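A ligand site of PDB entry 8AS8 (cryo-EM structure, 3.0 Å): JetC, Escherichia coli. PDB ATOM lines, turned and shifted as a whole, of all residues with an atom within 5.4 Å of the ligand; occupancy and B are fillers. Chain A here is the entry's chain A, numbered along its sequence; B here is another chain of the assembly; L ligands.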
ATOM      1  N   GLY A  24      32.365  13.836  24.885  1.00  0.00           N
ATOM      2  CA  GLY A  24      31.201  14.027  24.008  1.00  0.00           C
ATOM      3  C   GLY A  24      31.365  15.265  23.132  1.00  0.00           C
ATOM      4  O   GLY A  24      32.327  15.296  22.334  1.00  0.00           O
ATOM      5  N   GLY A  25      30.457  16.240  23.267  1.00  0.00           N
ATOM      6  CA  GLY A  25      30.556  17.481  22.481  1.00  0.00           C
ATOM      7  C   GLY A  25      31.227  18.587  23.266  1.00  0.00           C
ATOM      8  O   GLY A  25      31.281  19.723  22.756  1.00  0.00           O
ATOM      9  N   PRO A  44      18.186  23.556  24.918  1.00  0.00           N
ATOM     10  CA  PRO A  44      17.503  23.000  23.743  1.00  0.00           C
ATOM     11  C   PRO A  44      17.928  21.558  23.502  1.00  0.00           C
ATOM     12  O   PRO A  44      19.063  21.172  23.751  1.00  0.00           O
ATOM     13  CB  PRO A  44      17.970  23.916  22.601  1.00  0.00           C
ATOM     14  CG  PRO A  44      19.222  24.544  23.090  1.00  0.00           C
ATOM     15  CD  PRO A  44      19.073  24.680  24.569  1.00  0.00           C
ATOM     16  N   THR A  45      16.976  20.749  23.036  1.00  0.00           N
ATOM     17  CA  THR A  45      17.258  19.295  22.814  1.00  0.00           C
ATOM     18  C   THR A  45      18.361  19.139  21.768  1.00  0.00           C
ATOM     19  O   THR A  45      18.185  19.631  20.637  1.00  0.00           O
ATOM     20  CB  THR A  45      15.969  18.543  22.463  1.00  0.00           C
ATOM     21  OG1 THR A  45      16.316  17.206  22.078  1.00  0.00           O
ATOM     22  CG2 THR A  45      15.170  19.201  21.362  1.00  0.00           C
ATOM     23  N   GLY A  46      19.466  18.475  22.128  1.00  0.00           N
ATOM     24  CA  GLY A  46      20.580  18.249  21.183  1.00  0.00           C
ATOM     25  C   GLY A  46      21.808  19.066  21.551  1.00  0.00           C
ATOM     26  O   GLY A  46      22.562  19.436  20.624  1.00  0.00           O
ATOM     27  N   SER A  47      22.021  19.326  22.839  1.00  0.00           N
ATOM     28  CA  SER A  47      23.228  20.071  23.292  1.00  0.00           C
ATOM     29  C   SER A  47      24.210  19.107  23.965  1.00  0.00           C
ATOM     30  O   SER A  47      24.967  18.443  23.232  1.00  0.00           O
ATOM     31  CB  SER A  47      22.849  21.206  24.219  1.00  0.00           C
ATOM     32  OG  SER A  47      21.775  20.825  25.072  1.00  0.00           O
ATOM     33  N   GLY A  48      24.187  19.033  25.299  1.00  0.00           N
ATOM     34  CA  GLY A  48      25.080  18.099  26.035  1.00  0.00           C
ATOM     35  C   GLY A  48      24.501  17.744  27.384  1.00  0.00           C
ATOM     36  O   GLY A  48      25.293  17.481  28.320  1.00  0.00           O
ATOM     37  N   LYS A  49      23.172  17.726  27.509  1.00  0.00           N
ATOM     38  CA  LYS A  49      22.499  17.412  28.794  1.00  0.00           C
ATOM     39  C   LYS A  49      22.606  15.906  29.063  1.00  0.00           C
ATOM     40  O   LYS A  49      22.947  15.536  30.208  1.00  0.00           O
ATOM     41  CB  LYS A  49      21.052  17.904  28.774  1.00  0.00           C
ATOM     42  CG  LYS A  49      20.875  19.401  28.566  1.00  0.00           C
ATOM     43  CD  LYS A  49      19.444  19.826  28.357  1.00  0.00           C
ATOM     44  CE  LYS A  49      18.674  18.903  27.445  1.00  0.00           C
ATOM     45  NZ  LYS A  49      19.190  18.932  26.063  1.00  0.00           N
ATOM     46  N   THR A  50      22.339  15.078  28.056  1.00  0.00           N
ATOM     47  CA  THR A  50      22.495  13.606  28.212  1.00  0.00           C
ATOM     48  C   THR A  50      23.991  13.279  28.319  1.00  0.00           C
ATOM     49  O   THR A  50      24.326  12.312  29.027  1.00  0.00           O
ATOM     50  CB  THR A  50      21.820  12.846  27.066  1.00  0.00           C
ATOM     51  OG1 THR A  50      20.813  11.993  27.623  1.00  0.00           O
ATOM     52  CG2 THR A  50      22.783  12.013  26.241  1.00  0.00           C
ATOM     53  N   THR A  51      24.835  14.067  27.642  1.00  0.00           N
ATOM     54  CA  THR A  51      26.306  13.852  27.703  1.00  0.00           C
ATOM     55  C   THR A  51      26.780  14.024  29.151  1.00  0.00           C
ATOM     56  O   THR A  51      27.618  13.213  29.590  1.00  0.00           O
ATOM     57  CB  THR A  51      27.012  14.818  26.748  1.00  0.00           C
ATOM     58  OG1 THR A  51      26.609  14.500  25.410  1.00  0.00           O
ATOM     59  CG2 THR A  51      28.520  14.773  26.844  1.00  0.00           C
ATOM     60  N   ASN A  67      22.663   7.012  27.600  1.00  0.00           N
ATOM     61  CA  ASN A  67      21.443   7.494  26.904  1.00  0.00           C
ATOM     62  C   ASN A  67      20.235   6.635  27.279  1.00  0.00           C
ATOM     63  O   ASN A  67      19.374   6.434  26.413  1.00  0.00           O
ATOM     64  CB  ASN A  67      21.640   7.585  25.385  1.00  0.00           C
ATOM     65  CG  ASN A  67      21.244   8.931  24.818  1.00  0.00           C
ATOM     66  OD1 ASN A  67      20.311   9.562  25.305  1.00  0.00           O
ATOM     67  ND2 ASN A  67      21.955   9.382  23.792  1.00  0.00           N
ATOM     68  N   SER A  70      16.331   7.881  26.484  1.00  0.00           N
ATOM     69  CA  SER A  70      15.700   7.761  25.172  1.00  0.00           C
ATOM     70  C   SER A  70      15.825   6.384  24.544  1.00  0.00           C
ATOM     71  O   SER A  70      14.977   6.005  23.735  1.00  0.00           O
ATOM     72  CB  SER A  70      16.272   8.798  24.202  1.00  0.00           C
ATOM     73  OG  SER A  70      17.589   8.460  23.819  1.00  0.00           O
ATOM     74  N   ARG A  78      25.087   4.705  22.150  1.00  0.00           N
ATOM     75  CA  ARG A  78      26.385   5.312  22.541  1.00  0.00           C
ATOM     76  C   ARG A  78      27.210   4.388  23.423  1.00  0.00           C
ATOM     77  O   ARG A  78      26.633   3.450  24.019  1.00  0.00           O
ATOM     78  CB  ARG A  78      26.143   6.642  23.273  1.00  0.00           C
ATOM     79  CG  ARG A  78      26.234   7.867  22.381  1.00  0.00           C
ATOM     80  CD  ARG A  78      25.713   9.117  23.058  1.00  0.00           C
ATOM     81  NE  ARG A  78      24.782   9.847  22.204  1.00  0.00           N
ATOM     82  CZ  ARG A  78      24.502  11.151  22.332  1.00  0.00           C
ATOM     83  NH1 ARG A  78      25.081  11.855  23.288  1.00  0.00           N
ATOM     84  NH2 ARG A  78      23.643  11.717  21.513  1.00  0.00           N
ATOM     85  N   ASP A  79      28.518   4.650  23.507  1.00  0.00           N
ATOM     86  CA  ASP A  79      29.413   3.844  24.373  1.00  0.00           C
ATOM     87  C   ASP A  79      30.516   4.782  24.870  1.00  0.00           C
ATOM     88  O   ASP A  79      30.488   5.976  24.504  1.00  0.00           O
ATOM     89  CB  ASP A  79      29.982   2.642  23.627  1.00  0.00           C
ATOM     90  CG  ASP A  79      30.342   2.941  22.173  1.00  0.00           C
ATOM     91  OD1 ASP A  79      29.476   2.703  21.307  1.00  0.00           O
ATOM     92  OD2 ASP A  79      31.465   3.403  21.941  1.00  0.00           O
ATOM     93  N   SER A  82      32.757   6.172  21.945  1.00  0.00           N
ATOM     94  CA  SER A  82      32.136   7.254  21.140  1.00  0.00           C
ATOM     95  C   SER A  82      32.098   8.566  21.922  1.00  0.00           C
ATOM     96  O   SER A  82      32.026   9.636  21.285  1.00  0.00           O
ATOM     97  CB  SER A  82      30.751   6.850  20.692  1.00  0.00           C
ATOM     98  OG  SER A  82      29.778   7.196  21.664  1.00  0.00           O
ATOM     99  N   TYR A  83      32.146   8.495  23.254  1.00  0.00           N
ATOM    100  CA  TYR A  83      32.180   9.732  24.084  1.00  0.00           C
ATOM    101  C   TYR A  83      33.606  10.282  24.089  1.00  0.00           C
ATOM    102  O   TYR A  83      33.778  11.501  23.981  1.00  0.00           O
ATOM    103  CB  TYR A  83      31.622   9.459  25.485  1.00  0.00           C
ATOM    104  CG  TYR A  83      30.189   9.901  25.651  1.00  0.00           C
ATOM    105  CD1 TYR A  83      29.851  11.240  25.584  1.00  0.00           C
ATOM    106  CD2 TYR A  83      29.178   8.983  25.859  1.00  0.00           C
ATOM    107  CE1 TYR A  83      28.543  11.662  25.726  1.00  0.00           C
ATOM    108  CE2 TYR A  83      27.863   9.381  25.998  1.00  0.00           C
ATOM    109  CZ  TYR A  83      27.541  10.724  25.933  1.00  0.00           C
ATOM    110  OH  TYR A  83      26.245  11.141  26.081  1.00  0.00           O
ATOM    111  N   GLY A  86      34.219  11.644  20.676  1.00  0.00           N
ATOM    112  CA  GLY A  86      33.302  12.703  20.292  1.00  0.00           C
ATOM    113  C   GLY A  86      32.597  12.470  18.975  1.00  0.00           C
ATOM    114  O   GLY A  86      32.435  13.411  18.196  1.00  0.00           O
ATOM    115  N   VAL A  87      32.171  11.227  18.737  1.00  0.00           N
ATOM    116  CA  VAL A  87      31.412  10.923  17.487  1.00  0.00           C
ATOM    117  C   VAL A  87      30.115  11.747  17.499  1.00  0.00           C
ATOM    118  O   VAL A  87      29.623  12.050  18.601  1.00  0.00           O
ATOM    119  CB  VAL A  87      31.134   9.412  17.336  1.00  0.00           C
ATOM    120  CG1 VAL A  87      32.325   8.589  17.802  1.00  0.00           C
ATOM    121  CG2 VAL A  87      29.868   8.983  18.058  1.00  0.00           C
ATOM    122  N   SER A  88      29.597  12.099  16.323  1.00  0.00           N
ATOM    123  CA  SER A  88      28.338  12.878  16.234  1.00  0.00           C
ATOM    124  C   SER A  88      27.308  12.093  15.413  1.00  0.00           C
ATOM    125  O   SER A  88      26.774  12.660  14.450  1.00  0.00           O
ATOM    126  CB  SER A  88      28.573  14.248  15.648  1.00  0.00           C
ATOM    127  OG  SER A  88      27.866  15.238  16.375  1.00  0.00           O
ATOM    128  N   GLY A  89      27.070  10.829  15.782  1.00  0.00           N
ATOM    129  CA  GLY A  89      26.111   9.982  15.054  1.00  0.00           C
ATOM    130  C   GLY A  89      24.805  10.709  14.748  1.00  0.00           C
ATOM    131  O   GLY A  89      24.460  10.825  13.558  1.00  0.00           O
ATOM    132  N   PRO A  90      24.047  11.175  15.766  1.00  0.00           N
ATOM    133  CA  PRO A  90      22.768  11.853  15.549  1.00  0.00           C
ATOM    134  C   PRO A  90      22.856  13.053  14.585  1.00  0.00           C
ATOM    135  O   PRO A  90      22.383  12.930  13.479  1.00  0.00           O
ATOM    136  CB  PRO A  90      22.392  12.368  16.945  1.00  0.00           C
ATOM    137  CG  PRO A  90      23.068  11.408  17.889  1.00  0.00           C
ATOM    138  CD  PRO A  90      24.366  11.037  17.192  1.00  0.00           C
ATOM    139  N   GLY A  91      23.423  14.176  15.040  1.00  0.00           N
ATOM    140  CA  GLY A  91      23.466  15.401  14.207  1.00  0.00           C
ATOM    141  C   GLY A  91      24.297  15.231  12.948  1.00  0.00           C
ATOM    142  O   GLY A  91      25.523  15.087  13.073  1.00  0.00           O
ATOM    143  N   GLU A1022      14.479  13.865  32.460  1.00  0.00           N
ATOM    144  CA  GLU A1022      13.108  14.038  31.887  1.00  0.00           C
ATOM    145  C   GLU A1022      12.164  13.116  32.657  1.00  0.00           C
ATOM    146  O   GLU A1022      11.449  12.333  32.006  1.00  0.00           O
ATOM    147  CB  GLU A1022      13.106  13.738  30.385  1.00  0.00           C
ATOM    148  CG  GLU A1022      13.542  14.916  29.544  1.00  0.00           C
ATOM    149  CD  GLU A1022      15.038  15.009  29.306  1.00  0.00           C
ATOM    150  OE1 GLU A1022      15.614  14.019  28.819  1.00  0.00           O
ATOM    151  OE2 GLU A1022      15.624  16.069  29.606  1.00  0.00           O
ATOM    152  N   ARG A1070      24.307  24.297  22.485  1.00  0.00           N
ATOM    153  CA  ARG A1070      25.266  23.887  21.431  1.00  0.00           C
ATOM    154  C   ARG A1070      25.461  25.034  20.434  1.00  0.00           C
ATOM    155  O   ARG A1070      24.452  25.650  20.036  1.00  0.00           O
ATOM    156  CB  ARG A1070      24.798  22.608  20.730  1.00  0.00           C
ATOM    157  CG  ARG A1070      25.926  21.789  20.128  1.00  0.00           C
ATOM    158  CD  ARG A1070      25.685  20.291  20.229  1.00  0.00           C
ATOM    159  NE  ARG A1070      26.925  19.524  20.223  1.00  0.00           N
ATOM    160  CZ  ARG A1070      27.224  18.579  19.340  1.00  0.00           C
ATOM    161  NH1 ARG A1070      26.362  18.285  18.381  1.00  0.00           N
ATOM    162  NH2 ARG A1070      28.371  17.939  19.421  1.00  0.00           N
ATOM    163  N   SER A1075      29.300  21.942  22.453  1.00  0.00           N
ATOM    164  CA  SER A1075      28.400  22.181  23.561  1.00  0.00           C
ATOM    165  C   SER A1075      29.082  23.031  24.614  1.00  0.00           C
ATOM    166  O   SER A1075      30.281  22.892  24.855  1.00  0.00           O
ATOM    167  CB  SER A1075      27.921  20.864  24.179  1.00  0.00           C
ATOM    168  OG  SER A1075      27.438  19.988  23.179  1.00  0.00           O
ATOM    169  N   SER B 985      18.427  16.250  18.241  1.00  0.00           N
ATOM    170  CA  SER B 985      18.025  15.001  18.954  1.00  0.00           C
ATOM    171  C   SER B 985      16.732  14.440  18.368  1.00  0.00           C
ATOM    172  O   SER B 985      15.737  14.360  19.113  1.00  0.00           O
ATOM    173  CB  SER B 985      17.930  15.226  20.442  1.00  0.00           C
ATOM    174  OG  SER B 985      19.203  15.150  21.044  1.00  0.00           O
HETATM  175  P1  LIG L   1      19.567  14.839  24.764  1.00  0.00           P
HETATM  176  O1  LIG L   1      18.994  13.464  24.516  1.00  0.00           O
HETATM  177  O2  LIG L   1      19.712  15.157  26.235  1.00  0.00           O
HETATM  178  O3  LIG L   1      18.832  15.926  24.017  1.00  0.00           O
HETATM  179  P2  LIG L   1      22.300  15.823  24.335  1.00  0.00           P
HETATM  180  O4  LIG L   1      23.382  15.117  25.083  1.00  0.00           O
HETATM  181  O5  LIG L   1      21.778  17.105  24.879  1.00  0.00           O
HETATM  182  O6  LIG L   1      21.063  14.816  24.162  1.00  0.00           O
HETATM  183  O7  LIG L   1      22.745  16.030  22.801  1.00  0.00           O
HETATM  184  C1  LIG L   1      23.989  15.471  22.321  1.00  0.00           C
HETATM  185  C2  LIG L   1      24.373  16.134  21.015  1.00  0.00           C
HETATM  186  O8  LIG L   1      25.807  16.054  20.847  1.00  0.00           O
HETATM  187  C3  LIG L   1      23.810  15.502  19.737  1.00  0.00           C
HETATM  188  O9  LIG L   1      23.716  16.475  18.698  1.00  0.00           O
HETATM  189  C4  LIG L   1      24.842  14.426  19.413  1.00  0.00           C
HETATM  190  O10 LIG L   1      24.979  14.229  18.023  1.00  0.00           O
HETATM  191  C5  LIG L   1      26.142  14.976  20.010  1.00  0.00           C
HETATM  192  N1  LIG L   1      26.903  14.015  20.796  1.00  0.00           N
HETATM  193  C6  LIG L   1      27.563  14.264  21.971  1.00  0.00           C
HETATM  194  N2  LIG L   1      28.176  13.209  22.464  1.00  0.00           N
HETATM  195  C7  LIG L   1      27.911  12.206  21.552  1.00  0.00           C
HETATM  196  C8  LIG L   1      28.286  10.841  21.503  1.00  0.00           C
HETATM  197  N3  LIG L   1      29.040  10.260  22.426  1.00  0.00           N
HETATM  198  N4  LIG L   1      27.854  10.105  20.456  1.00  0.00           N
HETATM  199  C9  LIG L   1      27.095  10.714  19.530  1.00  0.00           C
HETATM  200  N5  LIG L   1      26.683  11.969  19.462  1.00  0.00           N
HETATM  201  C10 LIG L   1      27.131  12.674  20.519  1.00  0.00           C
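O3 of the ligand lies within hydrogen-bond range of OG of Ser 985 of chain B, at 3.1 Å.
The backbone NH of Gly 46 sits at hydrogen-bond distance from an oxygen (O3) of the ligand, 3.2 Å away.
OG of Ser 82 is in hydrogen-bond range of N3 of the ligand (3.2 Å).
The backbone NH (N) of Ser 47 is in hydrogen-bond range of an oxygen (O5) of the ligand.
The backbone NH of Lys 49 lies within hydrogen-bond range of an oxygen (O5) of the ligand.
An oxygen (O10) of the ligand is in hydrogen-bond range of the backbone NH of Gly 91 (3.4 Å).
An oxygen (O4) of the ligand sits at hydrogen-bond distance from the backbone NH (N) of Thr 51 (3.1 Å).
OG of Ser 88 lies within hydrogen-bond range of O10 of the ligand.
The side-chain hydroxyl of Thr 51 is in hydrogen-bond range of an oxygen (O4) of the ligand (3.3 Å).
An oxygen (O9) of the ligand is in hydrogen-bond range of the guanidinium group (NH1) of Arg 1070, 3.2 Å away.
An oxygen (O5) of the ligand is in salt-bridge range of the side-chain amino group (NZ) of Lys 49, at 3.4 Å.
The backbone NH (N) of Thr 50 lies within hydrogen-bond range of an oxygen (O4) of the ligand, 3.2 Å away.
OG1 of Thr 45 sits at hydrogen-bond distance from O3 of the ligand (3.4 Å).
N of Gly 48 sits at hydrogen-bond distance from O5 of the ligand (3.1 Å).
A nitrogen (N2) of the ligand sits close to the guanidinium group (NH1) of Arg 78 (3.5 Å).
The backbone carbonyl oxygen of Ser 82 is in hydrogen-bond range of a nitrogen (N3) of the ligand, at 3.3 Å.
O of Ser 47 sits at hydrogen-bond distance from OG of Ser 1075, at 2.9 Å.
The guanidinium group (NH1) of Arg 78 lies within hydrogen-bond range of the side-chain hydroxyl (OH) of Tyr 83.
OG1 of Thr 50 is in hydrogen-bond range of OD1 of Asn 67, 3.4 Å away.
OG of Ser 47 sits at hydrogen-bond distance from NZ of Lys 49 (3.4 Å).
The side-chain hydroxyl (OH) of Tyr 83 sits close to the side-chain hydroxyl (OG1) of Thr 51, 3.4 Å away.
OG of Ser 47 sits at hydrogen-bond distance from O of Pro 44 (3.0 Å).
The side-chain amino group (NZ) of Lys 49 is in hydrogen-bond range of the backbone carbonyl oxygen (O) of Pro 44, at 3.2 Å.
N of Ser 82 sits at hydrogen-bond distance from OD2 of Asp 79 (3.1 Å).
The backbone carbonyl oxygen (O) of Val 87 lies close to a nitrogen (N5) of the ligand.
Residues that only touch the ligand: Gly 24, Gly 25, Tyr 83, Gly 89 and Pro 90.
Hydrophobic or aromatic side chains within 4 Å of the ligand: Tyr 83, Val 87 and Pro 90.
Within 4 Å of the ligand: Gly 24, Gly 25, Thr 45, Gly 46, Ser 47, Gly 48, Lys 49, Thr 50, Thr 51, Arg 78, Ser 82, Tyr 83, Val 87, Ser 88, Gly 89, Pro 90, Gly 91, Arg 1070 and Ser 985 of chain B.
The nearest printed residue that does not touch the ligand is Asn 67 (4.2 Å).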
